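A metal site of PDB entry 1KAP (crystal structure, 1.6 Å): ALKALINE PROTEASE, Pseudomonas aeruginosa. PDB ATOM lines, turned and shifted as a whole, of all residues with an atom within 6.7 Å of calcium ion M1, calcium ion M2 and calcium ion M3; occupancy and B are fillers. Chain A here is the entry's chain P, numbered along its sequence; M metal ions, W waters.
The backbone NH (N) of Gly 378 is in hydrogen-bond range of the side-chain carboxylate (OD1) of Asp 403, 2.9 Å away. The backbone NH of Gly 360 sits at hydrogen-bond distance from the backbone carbonyl oxygen of Trp 377, at 2.8 Å. N of Gly 343 lies close to NE2 of Gln 310, 3.4 Å away. OD2 of Asp 403 is in hydrogen-bond range of N of Gly 379 (2.8 Å). The side-chain carboxylate (OD1) of Asp 347 sits at hydrogen-bond distance from the backbone NH (N) of Gln 310. OD2 of Asp 409 sits at hydrogen-bond distance from N of Val 405, 2.8 Å away.
Within 4 Å of calcium ion M1: Gly 379, Ala 380, Gly 381, Asp 383 and Asp 409. The nearest printed residue that does not touch calcium ion M1 is Gly 378 (4.1 Å).
Within 4 Å of calcium ion M2: Gly 361, Ala 362, Gly 363, Asp 365, Gly 378, Gly 379, Ala 380 and Asp 383. The nearest printed residue that does not touch calcium ion M2 is Gly 360 (4.3 Å).
The nearest printed residue that does not touch calcium ion M3 is Ser 344 (4.1 Å).
Calcium ion M1 is bound by OD2 of Asp 383 (2.3 Å), water W2 (2.3 Å), O of Gly 379 (2.4 Å), water W1 (2.4 Å), O of Gly 381 (2.4 Å) and OD1 of Asp 409 (2.5 Å). Calcium ion M1 has six donor atoms within binding distance.
Calcium ion M2 is bound by the backbone carbonyl oxygen of Gly 378 (2.3 Å), the backbone carbonyl oxygen of Gly 361 (2.3 Å), the side-chain carboxylate of Asp 365 (2.3 Å), the backbone carbonyl oxygen of Ala 380 (2.4 Å), the side-chain carboxylate of Asp 383 (2.4 Å) and the backbone carbonyl oxygen of Gly 363 (2.4 Å). Slightly farther from calcium ion M2 lies the side-chain carboxylate (OD2) of Asp 383 (3.1 Å).
Calcium ion M3 is bound by the backbone carbonyl oxygen (O) of Ala 362, the backbone carbonyl oxygen (O) of Gly 360, the backbone carbonyl oxygen (O) of Gly 343, the side-chain carboxylate (OD1) of Asp 365, the backbone carbonyl oxygen (O) of Gly 345 and the side-chain carboxylate (OD2) of Asp 347. Slightly farther from calcium ion M3 lies the side-chain carboxylate (OD2) of Asp 365 (3.1 Å).
Water W1 bridges OD2 of Asp 409 (2.6 Å) and OD1 of Asp 403 (3.1 Å).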
ATOM      1  N   GLN A 308       6.683  22.277  12.385  1.00  0.00           N
ATOM      2  CA  GLN A 308       6.268  23.558  12.945  1.00  0.00           C
ATOM      3  C   GLN A 308       4.935  23.963  12.343  1.00  0.00           C
ATOM      4  O   GLN A 308       4.536  23.458  11.285  1.00  0.00           O
ATOM      5  CB  GLN A 308       7.299  24.655  12.623  1.00  0.00           C
ATOM      6  CG  GLN A 308       8.709  24.418  13.134  1.00  0.00           C
ATOM      7  CD  GLN A 308       9.591  23.674  12.147  1.00  0.00           C
ATOM      8  OE1 GLN A 308       9.117  23.151  11.133  1.00  0.00           O
ATOM      9  NE2 GLN A 308      10.881  23.636  12.422  1.00  0.00           N
ATOM     10  N   GLN A 310       2.693  26.101  10.198  1.00  0.00           N
ATOM     11  CA  GLN A 310       2.990  26.890   9.025  1.00  0.00           C
ATOM     12  C   GLN A 310       1.813  27.702   8.515  1.00  0.00           C
ATOM     13  O   GLN A 310       0.667  27.397   8.837  1.00  0.00           O
ATOM     14  CB  GLN A 310       3.516  25.962   7.911  1.00  0.00           C
ATOM     15  CG  GLN A 310       4.661  25.070   8.372  1.00  0.00           C
ATOM     16  CD  GLN A 310       5.210  24.201   7.278  1.00  0.00           C
ATOM     17  OE1 GLN A 310       6.107  24.615   6.543  1.00  0.00           O
ATOM     18  NE2 GLN A 310       4.692  22.981   7.140  1.00  0.00           N
ATOM     19  N   GLY A 342       0.643  20.870   3.671  1.00  0.00           N
ATOM     20  CA  GLY A 342       1.144  21.294   4.971  1.00  0.00           C
ATOM     21  C   GLY A 342       1.929  20.164   5.650  1.00  0.00           C
ATOM     22  O   GLY A 342       2.073  19.064   5.092  1.00  0.00           O
ATOM     23  N   GLY A 343       2.440  20.443   6.849  1.00  0.00           N
ATOM     24  CA  GLY A 343       3.210  19.456   7.585  1.00  0.00           C
ATOM     25  C   GLY A 343       2.429  18.901   8.759  1.00  0.00           C
ATOM     26  O   GLY A 343       1.201  19.019   8.826  1.00  0.00           O
ATOM     27  N   SER A 344       3.132  18.347   9.739  1.00  0.00           N
ATOM     28  CA  SER A 344       2.454  17.775  10.896  1.00  0.00           C
ATOM     29  C   SER A 344       2.005  18.780  11.962  1.00  0.00           C
ATOM     30  O   SER A 344       1.409  18.396  12.973  1.00  0.00           O
ATOM     31  CB  SER A 344       3.298  16.656  11.501  1.00  0.00           C
ATOM     32  OG  SER A 344       4.510  17.148  12.046  1.00  0.00           O
ATOM     33  N   GLY A 345       2.304  20.058  11.785  1.00  0.00           N
ATOM     34  CA  GLY A 345       1.859  21.053  12.737  1.00  0.00           C
ATOM     35  C   GLY A 345       0.470  21.540  12.371  1.00  0.00           C
ATOM     36  O   GLY A 345      -0.126  21.062  11.409  1.00  0.00           O
ATOM     37  N   SER A 346      -0.065  22.483  13.136  1.00  0.00           N
ATOM     38  CA  SER A 346      -1.375  23.060  12.852  1.00  0.00           C
ATOM     39  C   SER A 346      -1.122  24.208  11.868  1.00  0.00           C
ATOM     40  O   SER A 346      -0.570  25.246  12.224  1.00  0.00           O
ATOM     41  CB  SER A 346      -2.030  23.524  14.155  1.00  0.00           C
ATOM     42  OG  SER A 346      -2.200  22.394  15.002  1.00  0.00           O
ATOM     43  N   ASP A 347      -1.515  23.995  10.624  1.00  0.00           N
ATOM     44  CA  ASP A 347      -1.251  24.933   9.536  1.00  0.00           C
ATOM     45  C   ASP A 347      -2.420  25.749   9.041  1.00  0.00           C
ATOM     46  O   ASP A 347      -3.578  25.401   9.253  1.00  0.00           O
ATOM     47  CB  ASP A 347      -0.696  24.152   8.349  1.00  0.00           C
ATOM     48  CG  ASP A 347       0.429  23.227   8.728  1.00  0.00           C
ATOM     49  OD1 ASP A 347       1.355  23.670   9.437  1.00  0.00           O
ATOM     50  OD2 ASP A 347       0.392  22.055   8.324  1.00  0.00           O
ATOM     51  N   LEU A 349      -3.663  27.117   5.439  1.00  0.00           N
ATOM     52  CA  LEU A 349      -3.461  26.981   3.995  1.00  0.00           C
ATOM     53  C   LEU A 349      -4.489  27.833   3.255  1.00  0.00           C
ATOM     54  O   LEU A 349      -5.710  27.614   3.387  1.00  0.00           O
ATOM     55  CB  LEU A 349      -3.560  25.533   3.541  1.00  0.00           C
ATOM     56  CG  LEU A 349      -2.430  24.594   3.948  1.00  0.00           C
ATOM     57  CD1 LEU A 349      -2.775  23.912   5.247  1.00  0.00           C
ATOM     58  CD2 LEU A 349      -2.248  23.555   2.878  1.00  0.00           C
ATOM     59  N   LYS A 359      -3.747  20.190   1.153  1.00  0.00           N
ATOM     60  CA  LYS A 359      -3.707  19.062   2.070  1.00  0.00           C
ATOM     61  C   LYS A 359      -3.069  19.504   3.386  1.00  0.00           C
ATOM     62  O   LYS A 359      -1.912  19.917   3.412  1.00  0.00           O
ATOM     63  CB  LYS A 359      -2.921  17.905   1.469  1.00  0.00           C
ATOM     64  CG  LYS A 359      -3.494  17.401   0.181  1.00  0.00           C
ATOM     65  CD  LYS A 359      -2.799  16.148  -0.225  1.00  0.00           C
ATOM     66  CE  LYS A 359      -3.422  15.583  -1.477  1.00  0.00           C
ATOM     67  NZ  LYS A 359      -2.850  14.252  -1.833  1.00  0.00           N
ATOM     68  N   GLY A 360      -3.836  19.419   4.470  1.00  0.00           N
ATOM     69  CA  GLY A 360      -3.350  19.852   5.755  1.00  0.00           C
ATOM     70  C   GLY A 360      -2.405  18.907   6.455  1.00  0.00           C
ATOM     71  O   GLY A 360      -1.549  19.365   7.211  1.00  0.00           O
ATOM     72  N   GLY A 361      -2.530  17.616   6.209  1.00  0.00           N
ATOM     73  CA  GLY A 361      -1.682  16.642   6.895  1.00  0.00           C
ATOM     74  C   GLY A 361      -2.131  16.560   8.353  1.00  0.00           C
ATOM     75  O   GLY A 361      -3.257  16.946   8.678  1.00  0.00           O
ATOM     76  N   ALA A 362      -1.285  16.016   9.222  1.00  0.00           N
ATOM     77  CA  ALA A 362      -1.620  15.918  10.643  1.00  0.00           C
ATOM     78  C   ALA A 362      -1.709  17.330  11.232  1.00  0.00           C
ATOM     79  O   ALA A 362      -1.241  18.294  10.619  1.00  0.00           O
ATOM     80  CB  ALA A 362      -0.566  15.080  11.385  1.00  0.00           C
ATOM     81  N   GLY A 363      -2.262  17.441  12.426  1.00  0.00           N
ATOM     82  CA  GLY A 363      -2.405  18.733  13.067  1.00  0.00           C
ATOM     83  C   GLY A 363      -3.781  19.306  12.778  1.00  0.00           C
ATOM     84  O   GLY A 363      -4.472  18.846  11.877  1.00  0.00           O
ATOM     85  N   ASN A 364      -4.180  20.291  13.555  1.00  0.00           N
ATOM     86  CA  ASN A 364      -5.470  20.956  13.405  1.00  0.00           C
ATOM     87  C   ASN A 364      -5.290  22.127  12.447  1.00  0.00           C
ATOM     88  O   ASN A 364      -4.942  23.237  12.844  1.00  0.00           O
ATOM     89  CB  ASN A 364      -5.982  21.440  14.768  1.00  0.00           C
ATOM     90  CG  ASN A 364      -6.297  20.284  15.725  1.00  0.00           C
ATOM     91  OD1 ASN A 364      -6.264  19.100  15.368  1.00  0.00           O
ATOM     92  ND2 ASN A 364      -6.607  20.633  16.957  1.00  0.00           N
ATOM     93  N   ASP A 365      -5.551  21.867  11.173  1.00  0.00           N
ATOM     94  CA  ASP A 365      -5.355  22.840  10.118  1.00  0.00           C
ATOM     95  C   ASP A 365      -6.580  23.668   9.776  1.00  0.00           C
ATOM     96  O   ASP A 365      -7.715  23.251  10.028  1.00  0.00           O
ATOM     97  CB  ASP A 365      -4.860  22.116   8.867  1.00  0.00           C
ATOM     98  CG  ASP A 365      -3.690  21.187   9.163  1.00  0.00           C
ATOM     99  OD1 ASP A 365      -2.608  21.678   9.516  1.00  0.00           O
ATOM    100  OD2 ASP A 365      -3.851  19.961   9.039  1.00  0.00           O
ATOM    101  N   LEU A 367      -8.144  25.530   6.442  1.00  0.00           N
ATOM    102  CA  LEU A 367      -8.019  25.578   4.990  1.00  0.00           C
ATOM    103  C   LEU A 367      -9.015  26.556   4.389  1.00  0.00           C
ATOM    104  O   LEU A 367     -10.174  26.615   4.790  1.00  0.00           O
ATOM    105  CB  LEU A 367      -8.210  24.156   4.384  1.00  0.00           C
ATOM    106  CG  LEU A 367      -7.162  23.069   4.713  1.00  0.00           C
ATOM    107  CD1 LEU A 367      -7.494  22.417   6.063  1.00  0.00           C
ATOM    108  CD2 LEU A 367      -7.157  21.997   3.644  1.00  0.00           C
ATOM    109  N   TRP A 377      -8.314  18.539   1.635  1.00  0.00           N
ATOM    110  CA  TRP A 377      -8.021  17.399   2.489  1.00  0.00           C
ATOM    111  C   TRP A 377      -7.538  17.932   3.830  1.00  0.00           C
ATOM    112  O   TRP A 377      -6.489  18.575   3.893  1.00  0.00           O
ATOM    113  CB  TRP A 377      -6.913  16.574   1.879  1.00  0.00           C
ATOM    114  CG  TRP A 377      -7.181  16.071   0.518  1.00  0.00           C
ATOM    115  CD1 TRP A 377      -7.095  16.769  -0.682  1.00  0.00           C
ATOM    116  CD2 TRP A 377      -7.512  14.734   0.171  1.00  0.00           C
ATOM    117  NE1 TRP A 377      -7.332  15.925  -1.730  1.00  0.00           N
ATOM    118  CE2 TRP A 377      -7.591  14.668  -1.243  1.00  0.00           C
ATOM    119  CE3 TRP A 377      -7.725  13.575   0.922  1.00  0.00           C
ATOM    120  CZ2 TRP A 377      -7.887  13.490  -1.918  1.00  0.00           C
ATOM    121  CZ3 TRP A 377      -8.024  12.403   0.254  1.00  0.00           C
ATOM    122  CH2 TRP A 377      -8.097  12.365  -1.151  1.00  0.00           C
ATOM    123  N   GLY A 378      -8.283  17.682   4.905  1.00  0.00           N
ATOM    124  CA  GLY A 378      -7.844  18.137   6.203  1.00  0.00           C
ATOM    125  C   GLY A 378      -6.792  17.220   6.826  1.00  0.00           C
ATOM    126  O   GLY A 378      -5.934  17.672   7.588  1.00  0.00           O
ATOM    127  N   GLY A 379      -6.813  15.952   6.439  1.00  0.00           N
ATOM    128  CA  GLY A 379      -5.894  14.972   7.014  1.00  0.00           C
ATOM    129  C   GLY A 379      -6.314  14.672   8.453  1.00  0.00           C
ATOM    130  O   GLY A 379      -7.447  14.954   8.856  1.00  0.00           O
ATOM    131  N   ALA A 380      -5.416  14.070   9.229  1.00  0.00           N
ATOM    132  CA  ALA A 380      -5.712  13.760  10.632  1.00  0.00           C
ATOM    133  C   ALA A 380      -5.869  15.056  11.401  1.00  0.00           C
ATOM    134  O   ALA A 380      -5.397  16.106  10.971  1.00  0.00           O
ATOM    135  CB  ALA A 380      -4.579  12.929  11.231  1.00  0.00           C
ATOM    136  N   GLY A 381      -6.523  14.983  12.549  1.00  0.00           N
ATOM    137  CA  GLY A 381      -6.725  16.164  13.371  1.00  0.00           C
ATOM    138  C   GLY A 381      -8.044  16.842  13.086  1.00  0.00           C
ATOM    139  O   GLY A 381      -8.760  16.474  12.153  1.00  0.00           O
ATOM    140  N   ALA A 382      -8.379  17.828  13.909  1.00  0.00           N
ATOM    141  CA  ALA A 382      -9.616  18.579  13.775  1.00  0.00           C
ATOM    142  C   ALA A 382      -9.376  19.767  12.822  1.00  0.00           C
ATOM    143  O   ALA A 382      -8.828  20.801  13.233  1.00  0.00           O
ATOM    144  CB  ALA A 382     -10.062  19.067  15.142  1.00  0.00           C
ATOM    145  N   ASP A 383      -9.816  19.617  11.586  1.00  0.00           N
ATOM    146  CA  ASP A 383      -9.612  20.650  10.571  1.00  0.00           C
ATOM    147  C   ASP A 383     -10.828  21.513  10.303  1.00  0.00           C
ATOM    148  O   ASP A 383     -11.964  21.059  10.418  1.00  0.00           O
ATOM    149  CB  ASP A 383      -9.122  19.981   9.302  1.00  0.00           C
ATOM    150  CG  ASP A 383      -7.945  19.063   9.578  1.00  0.00           C
ATOM    151  OD1 ASP A 383      -6.871  19.565   9.959  1.00  0.00           O
ATOM    152  OD2 ASP A 383      -8.099  17.825   9.454  1.00  0.00           O
ATOM    153  N   PHE A 385     -12.650  24.065   7.487  1.00  0.00           N
ATOM    154  CA  PHE A 385     -12.726  24.509   6.098  1.00  0.00           C
ATOM    155  C   PHE A 385     -13.508  25.822   6.119  1.00  0.00           C
ATOM    156  O   PHE A 385     -14.691  25.853   6.447  1.00  0.00           O
ATOM    157  CB  PHE A 385     -13.388  23.425   5.250  1.00  0.00           C
ATOM    158  CG  PHE A 385     -12.706  22.100   5.378  1.00  0.00           C
ATOM    159  CD1 PHE A 385     -11.638  21.762   4.541  1.00  0.00           C
ATOM    160  CD2 PHE A 385     -13.082  21.192   6.383  1.00  0.00           C
ATOM    161  CE1 PHE A 385     -10.945  20.557   4.705  1.00  0.00           C
ATOM    162  CE2 PHE A 385     -12.392  19.992   6.554  1.00  0.00           C
ATOM    163  CZ  PHE A 385     -11.322  19.671   5.719  1.00  0.00           C
ATOM    164  N   ASP A 403     -12.060  14.273   2.818  1.00  0.00           N
ATOM    165  CA  ASP A 403     -11.870  13.359   3.935  1.00  0.00           C
ATOM    166  C   ASP A 403     -12.527  13.895   5.207  1.00  0.00           C
ATOM    167  O   ASP A 403     -11.975  13.803   6.307  1.00  0.00           O
ATOM    168  CB  ASP A 403     -10.357  13.130   4.162  1.00  0.00           C
ATOM    169  CG  ASP A 403      -9.592  14.423   4.539  1.00  0.00           C
ATOM    170  OD1 ASP A 403     -10.167  15.527   4.546  1.00  0.00           O
ATOM    171  OD2 ASP A 403      -8.389  14.327   4.841  1.00  0.00           O
ATOM    172  N   PHE A 404     -13.728  14.440   5.048  1.00  0.00           N
ATOM    173  CA  PHE A 404     -14.442  15.022   6.156  1.00  0.00           C
ATOM    174  C   PHE A 404     -14.836  14.012   7.232  1.00  0.00           C
ATOM    175  O   PHE A 404     -15.400  12.965   6.932  1.00  0.00           O
ATOM    176  CB  PHE A 404     -15.689  15.753   5.658  1.00  0.00           C
ATOM    177  CG  PHE A 404     -16.258  16.719   6.650  1.00  0.00           C
ATOM    178  CD1 PHE A 404     -15.784  18.030   6.720  1.00  0.00           C
ATOM    179  CD2 PHE A 404     -17.254  16.311   7.550  1.00  0.00           C
ATOM    180  CE1 PHE A 404     -16.285  18.921   7.669  1.00  0.00           C
ATOM    181  CE2 PHE A 404     -17.748  17.190   8.484  1.00  0.00           C
ATOM    182  CZ  PHE A 404     -17.273  18.501   8.554  1.00  0.00           C
ATOM    183  N   VAL A 405     -14.544  14.346   8.477  1.00  0.00           N
ATOM    184  CA  VAL A 405     -14.881  13.472   9.601  1.00  0.00           C
ATOM    185  C   VAL A 405     -15.773  14.234  10.582  1.00  0.00           C
ATOM    186  O   VAL A 405     -15.323  15.174  11.251  1.00  0.00           O
ATOM    187  CB  VAL A 405     -13.615  12.978  10.335  1.00  0.00           C
ATOM    188  CG1 VAL A 405     -13.993  12.143  11.544  1.00  0.00           C
ATOM    189  CG2 VAL A 405     -12.750  12.175   9.386  1.00  0.00           C
ATOM    190  N   GLN A 408     -15.199  15.945  14.246  1.00  0.00           N
ATOM    191  CA  GLN A 408     -13.791  16.351  14.315  1.00  0.00           C
ATOM    192  C   GLN A 408     -13.583  17.599  13.464  1.00  0.00           C
ATOM    193  O   GLN A 408     -13.172  18.635  13.980  1.00  0.00           O
ATOM    194  CB  GLN A 408     -12.862  15.246  13.833  1.00  0.00           C
ATOM    195  CG  GLN A 408     -12.132  14.533  14.968  1.00  0.00           C
ATOM    196  CD  GLN A 408     -10.738  14.071  14.555  1.00  0.00           C
ATOM    197  OE1 GLN A 408     -10.575  13.391  13.535  1.00  0.00           O
ATOM    198  NE2 GLN A 408      -9.731  14.435  15.343  1.00  0.00           N
ATOM    199  N   ASP A 409     -13.883  17.495  12.182  1.00  0.00           N
ATOM    200  CA  ASP A 409     -13.726  18.636  11.278  1.00  0.00           C
ATOM    201  C   ASP A 409     -14.932  19.567  11.349  1.00  0.00           C
ATOM    202  O   ASP A 409     -15.982  19.196  11.886  1.00  0.00           O
ATOM    203  CB  ASP A 409     -13.530  18.156   9.839  1.00  0.00           C
ATOM    204  CG  ASP A 409     -12.372  17.201   9.693  1.00  0.00           C
ATOM    205  OD1 ASP A 409     -11.336  17.366  10.363  1.00  0.00           O
ATOM    206  OD2 ASP A 409     -12.499  16.282   8.889  1.00  0.00           O
HETATM  207 CA    CA M   1      -9.357  15.987   9.828  1.00  0.00          CA
HETATM  208 CA    CA M   2      -5.049  18.051   9.682  1.00  0.00          CA
HETATM  209 CA    CA M   3      -0.801  20.162   9.288  1.00  0.00          CA
HETATM  210  O   HOH W   1     -10.233  16.039   7.563  1.00  0.00           O
HETATM  211  O   HOH W   2      -9.914  13.890  10.711  1.00  0.00           O
